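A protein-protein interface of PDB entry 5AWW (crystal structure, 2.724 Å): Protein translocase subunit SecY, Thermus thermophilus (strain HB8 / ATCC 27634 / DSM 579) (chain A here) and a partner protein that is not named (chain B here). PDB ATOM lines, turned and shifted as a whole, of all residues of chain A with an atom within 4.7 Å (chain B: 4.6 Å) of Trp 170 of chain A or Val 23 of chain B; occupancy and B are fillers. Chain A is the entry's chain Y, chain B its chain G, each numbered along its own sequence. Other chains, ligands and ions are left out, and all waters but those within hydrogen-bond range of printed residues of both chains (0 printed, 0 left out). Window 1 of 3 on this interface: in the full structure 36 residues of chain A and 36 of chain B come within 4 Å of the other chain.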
ATOM      1  N   ARG A 116      21.191  14.941 -17.075  1.00  0.00           N
ATOM      2  CA  ARG A 116      22.076  13.793 -16.883  1.00  0.00           C
ATOM      3  C   ARG A 116      23.085  14.051 -15.761  1.00  0.00           C
ATOM      4  O   ARG A 116      23.234  13.237 -14.842  1.00  0.00           O
ATOM      5  CB  ARG A 116      22.801  13.461 -18.190  1.00  0.00           C
ATOM      6  CG  ARG A 116      21.852  13.178 -19.347  1.00  0.00           C
ATOM      7  CD  ARG A 116      22.544  13.237 -20.701  1.00  0.00           C
ATOM      8  NE  ARG A 116      23.142  11.962 -21.084  1.00  0.00           N
ATOM      9  CZ  ARG A 116      24.450  11.724 -21.108  1.00  0.00           C
ATOM     10  NH1 ARG A 116      25.308  12.679 -20.775  1.00  0.00           N
ATOM     11  NH2 ARG A 116      24.899  10.531 -21.470  1.00  0.00           N
ATOM     12  N   ALA A 166      25.710   6.049 -13.323  1.00  0.00           N
ATOM     13  CA  ALA A 166      26.298   6.504 -14.577  1.00  0.00           C
ATOM     14  C   ALA A 166      26.168   5.386 -15.611  1.00  0.00           C
ATOM     15  O   ALA A 166      25.591   5.582 -16.688  1.00  0.00           O
ATOM     16  CB  ALA A 166      27.749   6.900 -14.387  1.00  0.00           C
ATOM     17  N   LEU A 167      26.684   4.210 -15.261  1.00  0.00           N
ATOM     18  CA  LEU A 167      26.590   3.046 -16.135  1.00  0.00           C
ATOM     19  C   LEU A 167      25.139   2.735 -16.509  1.00  0.00           C
ATOM     20  O   LEU A 167      24.849   2.411 -17.657  1.00  0.00           O
ATOM     21  CB  LEU A 167      27.237   1.823 -15.474  1.00  0.00           C
ATOM     22  CG  LEU A 167      27.395   0.555 -16.322  1.00  0.00           C
ATOM     23  CD1 LEU A 167      28.241   0.823 -17.558  1.00  0.00           C
ATOM     24  CD2 LEU A 167      27.998  -0.574 -15.500  1.00  0.00           C
ATOM     25  N   LEU A 168      24.228   2.857 -15.549  1.00  0.00           N
ATOM     26  CA  LEU A 168      22.824   2.519 -15.789  1.00  0.00           C
ATOM     27  C   LEU A 168      22.125   3.517 -16.716  1.00  0.00           C
ATOM     28  O   LEU A 168      21.346   3.121 -17.585  1.00  0.00           O
ATOM     29  CB  LEU A 168      22.068   2.426 -14.465  1.00  0.00           C
ATOM     30  CG  LEU A 168      20.649   1.870 -14.573  1.00  0.00           C
ATOM     31  CD1 LEU A 168      20.658   0.534 -15.291  1.00  0.00           C
ATOM     32  CD2 LEU A 168      20.035   1.731 -13.198  1.00  0.00           C
ATOM     33  N   LEU A 169      22.394   4.804 -16.518  1.00  0.00           N
ATOM     34  CA  LEU A 169      21.904   5.846 -17.417  1.00  0.00           C
ATOM     35  C   LEU A 169      22.418   5.609 -18.833  1.00  0.00           C
ATOM     36  O   LEU A 169      21.670   5.723 -19.813  1.00  0.00           O
ATOM     37  CB  LEU A 169      22.333   7.230 -16.922  1.00  0.00           C
ATOM     38  CG  LEU A 169      22.092   8.408 -17.866  1.00  0.00           C
ATOM     39  CD1 LEU A 169      20.609   8.571 -18.159  1.00  0.00           C
ATOM     40  CD2 LEU A 169      22.672   9.689 -17.286  1.00  0.00           C
ATOM     41  N   TRP A 170      23.704   5.276 -18.929  1.00  0.00           N
ATOM     42  CA  TRP A 170      24.306   4.920 -20.206  1.00  0.00           C
ATOM     43  C   TRP A 170      23.551   3.760 -20.859  1.00  0.00           C
ATOM     44  O   TRP A 170      23.180   3.833 -22.031  1.00  0.00           O
ATOM     45  CB  TRP A 170      25.781   4.559 -20.018  1.00  0.00           C
ATOM     46  CG  TRP A 170      26.489   4.212 -21.292  1.00  0.00           C
ATOM     47  CD1 TRP A 170      27.129   5.074 -22.136  1.00  0.00           C
ATOM     48  CD2 TRP A 170      26.632   2.907 -21.867  1.00  0.00           C
ATOM     49  NE1 TRP A 170      27.660   4.387 -23.201  1.00  0.00           N
ATOM     50  CE2 TRP A 170      27.369   3.056 -23.059  1.00  0.00           C
ATOM     51  CE3 TRP A 170      26.209   1.630 -21.490  1.00  0.00           C
ATOM     52  CZ2 TRP A 170      27.692   1.975 -23.875  1.00  0.00           C
ATOM     53  CZ3 TRP A 170      26.529   0.558 -22.304  1.00  0.00           C
ATOM     54  CH2 TRP A 170      27.263   0.737 -23.482  1.00  0.00           C
ATOM     55  N   MET A 171      23.314   2.701 -20.088  1.00  0.00           N
ATOM     56  CA  MET A 171      22.616   1.515 -20.581  1.00  0.00           C
ATOM     57  C   MET A 171      21.214   1.846 -21.080  1.00  0.00           C
ATOM     58  O   MET A 171      20.773   1.335 -22.113  1.00  0.00           O
ATOM     59  CB  MET A 171      22.537   0.450 -19.486  1.00  0.00           C
ATOM     60  CG  MET A 171      23.875  -0.174 -19.127  1.00  0.00           C
ATOM     61  SD  MET A 171      23.792  -1.150 -17.616  1.00  0.00           S
ATOM     62  CE  MET A 171      22.443  -2.260 -18.016  1.00  0.00           C
ATOM     63  N   ALA A 172      20.519   2.701 -20.336  1.00  0.00           N
ATOM     64  CA  ALA A 172      19.187   3.148 -20.718  1.00  0.00           C
ATOM     65  C   ALA A 172      19.230   3.871 -22.057  1.00  0.00           C
ATOM     66  O   ALA A 172      18.432   3.588 -22.960  1.00  0.00           O
ATOM     67  CB  ALA A 172      18.603   4.052 -19.645  1.00  0.00           C
ATOM     68  N   GLU A 173      20.172   4.801 -22.185  1.00  0.00           N
ATOM     69  CA  GLU A 173      20.291   5.581 -23.410  1.00  0.00           C
ATOM     70  C   GLU A 173      20.658   4.697 -24.601  1.00  0.00           C
ATOM     71  O   GLU A 173      20.235   4.951 -25.732  1.00  0.00           O
ATOM     72  CB  GLU A 173      21.316   6.699 -23.224  1.00  0.00           C
ATOM     73  CG  GLU A 173      20.863   7.760 -22.230  1.00  0.00           C
ATOM     74  CD  GLU A 173      21.965   8.726 -21.855  1.00  0.00           C
ATOM     75  OE1 GLU A 173      21.648   9.787 -21.279  1.00  0.00           O
ATOM     76  OE2 GLU A 173      23.146   8.423 -22.130  1.00  0.00           O
ATOM     77  N   ARG A 174      21.427   3.645 -24.340  1.00  0.00           N
ATOM     78  CA  ARG A 174      21.795   2.705 -25.392  1.00  0.00           C
ATOM     79  C   ARG A 174      20.626   1.803 -25.770  1.00  0.00           C
ATOM     80  O   ARG A 174      20.548   1.337 -26.901  1.00  0.00           O
ATOM     81  CB  ARG A 174      22.997   1.857 -24.973  1.00  0.00           C
ATOM     82  CG  ARG A 174      24.273   2.657 -24.803  1.00  0.00           C
ATOM     83  CD  ARG A 174      24.582   3.493 -26.034  1.00  0.00           C
ATOM     84  NE  ARG A 174      25.239   4.743 -25.665  1.00  0.00           N
ATOM     85  CZ  ARG A 174      24.621   5.916 -25.570  1.00  0.00           C
ATOM     86  NH1 ARG A 174      23.328   6.005 -25.835  1.00  0.00           N
ATOM     87  NH2 ARG A 174      25.297   7.001 -25.220  1.00  0.00           N
ATOM     88  N   LEU B  19      34.476   6.622 -15.774  1.00  0.00           N
ATOM     89  CA  LEU B  19      33.213   6.118 -16.296  1.00  0.00           C
ATOM     90  C   LEU B  19      32.174   7.236 -16.347  1.00  0.00           C
ATOM     91  O   LEU B  19      31.424   7.360 -17.320  1.00  0.00           O
ATOM     92  CB  LEU B  19      32.709   4.956 -15.445  1.00  0.00           C
ATOM     93  CG  LEU B  19      31.727   4.005 -16.127  1.00  0.00           C
ATOM     94  CD1 LEU B  19      32.361   3.386 -17.363  1.00  0.00           C
ATOM     95  CD2 LEU B  19      31.275   2.929 -15.157  1.00  0.00           C
ATOM     96  N   VAL B  20      32.142   8.050 -15.296  1.00  0.00           N
ATOM     97  CA  VAL B  20      31.277   9.223 -15.259  1.00  0.00           C
ATOM     98  C   VAL B  20      31.576  10.151 -16.427  1.00  0.00           C
ATOM     99  O   VAL B  20      30.664  10.606 -17.121  1.00  0.00           O
ATOM    100  CB  VAL B  20      31.437  10.009 -13.945  1.00  0.00           C
ATOM    101  CG1 VAL B  20      30.569  11.262 -13.964  1.00  0.00           C
ATOM    102  CG2 VAL B  20      31.084   9.132 -12.763  1.00  0.00           C
ATOM    103  N   TYR B  21      32.860  10.422 -16.641  1.00  0.00           N
ATOM    104  CA  TYR B  21      33.286  11.292 -17.731  1.00  0.00           C
ATOM    105  C   TYR B  21      32.818  10.744 -19.074  1.00  0.00           C
ATOM    106  O   TYR B  21      32.223  11.465 -19.874  1.00  0.00           O
ATOM    107  CB  TYR B  21      34.808  11.462 -17.728  1.00  0.00           C
ATOM    108  CG  TYR B  21      35.324  12.374 -18.821  1.00  0.00           C
ATOM    109  CD1 TYR B  21      35.356  13.752 -18.645  1.00  0.00           C
ATOM    110  CD2 TYR B  21      35.779  11.857 -20.028  1.00  0.00           C
ATOM    111  CE1 TYR B  21      35.825  14.589 -19.642  1.00  0.00           C
ATOM    112  CE2 TYR B  21      36.248  12.686 -21.031  1.00  0.00           C
ATOM    113  CZ  TYR B  21      36.270  14.051 -20.833  1.00  0.00           C
ATOM    114  OH  TYR B  21      36.739  14.876 -21.831  1.00  0.00           O
ATOM    115  N   LEU B  22      33.077   9.461 -19.308  1.00  0.00           N
ATOM    116  CA  LEU B  22      32.705   8.817 -20.563  1.00  0.00           C
ATOM    117  C   LEU B  22      31.203   8.855 -20.813  1.00  0.00           C
ATOM    118  O   LEU B  22      30.764   9.110 -21.933  1.00  0.00           O
ATOM    119  CB  LEU B  22      33.191   7.368 -20.586  1.00  0.00           C
ATOM    120  CG  LEU B  22      34.696   7.138 -20.718  1.00  0.00           C
ATOM    121  CD1 LEU B  22      34.988   5.651 -20.721  1.00  0.00           C
ATOM    122  CD2 LEU B  22      35.236   7.796 -21.976  1.00  0.00           C
ATOM    123  N   VAL B  23      30.419   8.595 -19.771  1.00  0.00           N
ATOM    124  CA  VAL B  23      28.964   8.603 -19.905  1.00  0.00           C
ATOM    125  C   VAL B  23      28.443  10.014 -20.190  1.00  0.00           C
ATOM    126  O   VAL B  23      27.622  10.208 -21.089  1.00  0.00           O
ATOM    127  CB  VAL B  23      28.282   8.034 -18.642  1.00  0.00           C
ATOM    128  CG1 VAL B  23      26.781   8.267 -18.687  1.00  0.00           C
ATOM    129  CG2 VAL B  23      28.589   6.551 -18.504  1.00  0.00           C
ATOM    130  N   LEU B  24      28.933  10.994 -19.435  1.00  0.00           N
ATOM    131  CA  LEU B  24      28.533  12.386 -19.629  1.00  0.00           C
ATOM    132  C   LEU B  24      28.896  12.907 -21.022  1.00  0.00           C
ATOM    133  O   LEU B  24      28.126  13.645 -21.633  1.00  0.00           O
ATOM    134  CB  LEU B  24      29.167  13.276 -18.557  1.00  0.00           C
ATOM    135  CG  LEU B  24      28.514  13.192 -17.175  1.00  0.00           C
ATOM    136  CD1 LEU B  24      29.230  14.077 -16.168  1.00  0.00           C
ATOM    137  CD2 LEU B  24      27.045  13.568 -17.275  1.00  0.00           C
ATOM    138  N   VAL B  25      30.067  12.516 -21.517  1.00  0.00           N
ATOM    139  CA  VAL B  25      30.524  12.931 -22.841  1.00  0.00           C
ATOM    140  C   VAL B  25      29.631  12.368 -23.948  1.00  0.00           C
ATOM    141  O   VAL B  25      29.266  13.083 -24.886  1.00  0.00           O
ATOM    142  CB  VAL B  25      31.989  12.499 -23.091  1.00  0.00           C
ATOM    143  CG1 VAL B  25      32.323  12.539 -24.576  1.00  0.00           C
ATOM    144  CG2 VAL B  25      32.942  13.381 -22.302  1.00  0.00           C
ATOM    145  N   GLN B  26      29.275  11.092 -23.836  1.00  0.00           N
ATOM    146  CA  GLN B  26      28.414  10.460 -24.829  1.00  0.00           C
ATOM    147  C   GLN B  26      26.991  10.996 -24.741  1.00  0.00           C
ATOM    148  O   GLN B  26      26.096  10.329 -24.223  1.00  0.00           O
ATOM    149  CB  GLN B  26      28.412   8.941 -24.656  1.00  0.00           C
ATOM    150  CG  GLN B  26      29.777   8.300 -24.808  1.00  0.00           C
ATOM    151  CD  GLN B  26      29.709   6.789 -24.819  1.00  0.00           C
ATOM    152  OE1 GLN B  26      28.843   6.200 -25.466  1.00  0.00           O
ATOM    153  NE2 GLN B  26      30.621   6.150 -24.096  1.00  0.00           N
ATOM    154  N   TYR B  53      32.136   3.398 -26.615  1.00  0.00           N
ATOM    155  CA  TYR B  53      31.118   2.390 -26.329  1.00  0.00           C
ATOM    156  C   TYR B  53      31.780   1.154 -25.725  1.00  0.00           C
ATOM    157  O   TYR B  53      31.454   0.725 -24.607  1.00  0.00           O
ATOM    158  CB  TYR B  53      30.348   2.016 -27.601  1.00  0.00           C
ATOM    159  CG  TYR B  53      29.381   0.859 -27.444  1.00  0.00           C
ATOM    160  CD1 TYR B  53      29.795  -0.454 -27.644  1.00  0.00           C
ATOM    161  CD2 TYR B  53      28.050   1.081 -27.114  1.00  0.00           C
ATOM    162  CE1 TYR B  53      28.916  -1.512 -27.504  1.00  0.00           C
ATOM    163  CE2 TYR B  53      27.162   0.027 -26.973  1.00  0.00           C
ATOM    164  CZ  TYR B  53      27.599  -1.267 -27.169  1.00  0.00           C
ATOM    165  OH  TYR B  53      26.719  -2.315 -27.030  1.00  0.00           O
ATOM    166  N   THR B  56      33.390   1.844 -22.437  1.00  0.00           N
ATOM    167  CA  THR B  56      32.451   1.929 -21.331  1.00  0.00           C
ATOM    168  C   THR B  56      32.006   0.542 -20.906  1.00  0.00           C
ATOM    169  O   THR B  56      31.839   0.290 -19.718  1.00  0.00           O
ATOM    170  CB  THR B  56      31.209   2.773 -21.674  1.00  0.00           C
ATOM    171  OG1 THR B  56      30.809   2.515 -23.023  1.00  0.00           O
ATOM    172  CG2 THR B  56      31.511   4.252 -21.515  1.00  0.00           C
ATOM    173  N   VAL B  57      31.809  -0.357 -21.867  1.00  0.00           N
ATOM    174  CA  VAL B  57      31.448  -1.726 -21.508  1.00  0.00           C
ATOM    175  C   VAL B  57      32.563  -2.371 -20.686  1.00  0.00           C
ATOM    176  O   VAL B  57      32.322  -2.930 -19.603  1.00  0.00           O
ATOM    177  CB  VAL B  57      31.162  -2.591 -22.745  1.00  0.00           C
ATOM    178  CG1 VAL B  57      30.940  -4.036 -22.334  1.00  0.00           C
ATOM    179  CG2 VAL B  57      29.954  -2.055 -23.496  1.00  0.00           C
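NH2 of Arg 116 of chain A is in hydrogen-bond range of O of Val 23 of chain B, at 2.8 Å. The guanidinium group (NH1) of Arg 116 of chain A lies within hydrogen-bond range of the backbone carbonyl oxygen (O) of Leu 24 of chain B (3.1 Å). The backbone carbonyl oxygen of Gln 26 of chain B sits at hydrogen-bond distance from the guanidinium group of Arg 116 of chain A, at 3.0 Å. OE1 of Gln 26 of chain B is in hydrogen-bond range of NE1 of Trp 170 of chain A, 3.1 Å away.
The guanidinium group of Arg 116 of chain A is in salt-bridge range of the side-chain carboxylate of Glu 173 of chain A. O of Tyr 53 of chain B lies within hydrogen-bond range of OG1 of Thr 56 of chain B (2.5 Å).
Among the printed residues, pairs that only touch across the chains: Ala 166 of chain A with Val 23 of chain B (3.6 Å), Trp 170 of chain A with Val 23 of chain B (3.8 Å), Trp 170 of chain A with Tyr 53 of chain B (3.4 Å), Trp 170 of chain A with Thr 56 of chain B (3.3 Å), Trp 170 of chain A with Val 57 of chain B (3.9 Å) and Arg 174 of chain A with Gln 26 of chain B (3.6 Å).
Of chain B, only Val 23 (3.8 Å), Gln 26 (3.1 Å), Tyr 53 (3.4 Å), Thr 56 (3.3 Å) and Val 57 (3.9 Å) come within 4 Å of Trp 170 of chain A. Of the printed residues of chain A, Val 23 of chain B touches Arg 116 (2.8 Å), Ala 166 (3.6 Å) and Trp 170 (3.8 Å). Printed residues of chain B within 4 Å of Arg 174 of chain A: Gln 26. Printed residues of chain B within 4 Å of Arg 116 of chain A: Val 23 (2.8 Å), Leu 24 (3.1 Å) and Gln 26 (3.0 Å). Of the printed residues of chain A, Thr 56 of chain B touches Trp 170 (3.3 Å). Of the printed residues of chain B, Ala 166 of chain A touches Val 23 (3.6 Å). Printed residues of chain A within 4 Å of Leu 24 of chain B: Arg 116. Met 171 of chain A touches none of the printed residues of chain B. Tyr 21 of chain B touches none of the printed residues of chain A. The nearest residue of chain A that does not touch Val 23 of chain B is Leu 167 of chain A (4.4 Å).
Of the 10 printed residues of chain A, 4 touch a printed residue of chain B. Hydrophobic or aromatic side chains of chain A within 4 Å of the printed part of chain B: Trp 170. Of the 11 printed residues of chain B, 6 touch a printed residue of chain A. Hydrophobic or aromatic side chains of chain B that line the printed part of chain A: Val 23, Tyr 53 and Val 57. Along chain B the printed residues that touch a printed residue of chain A span positions 23 to 57.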
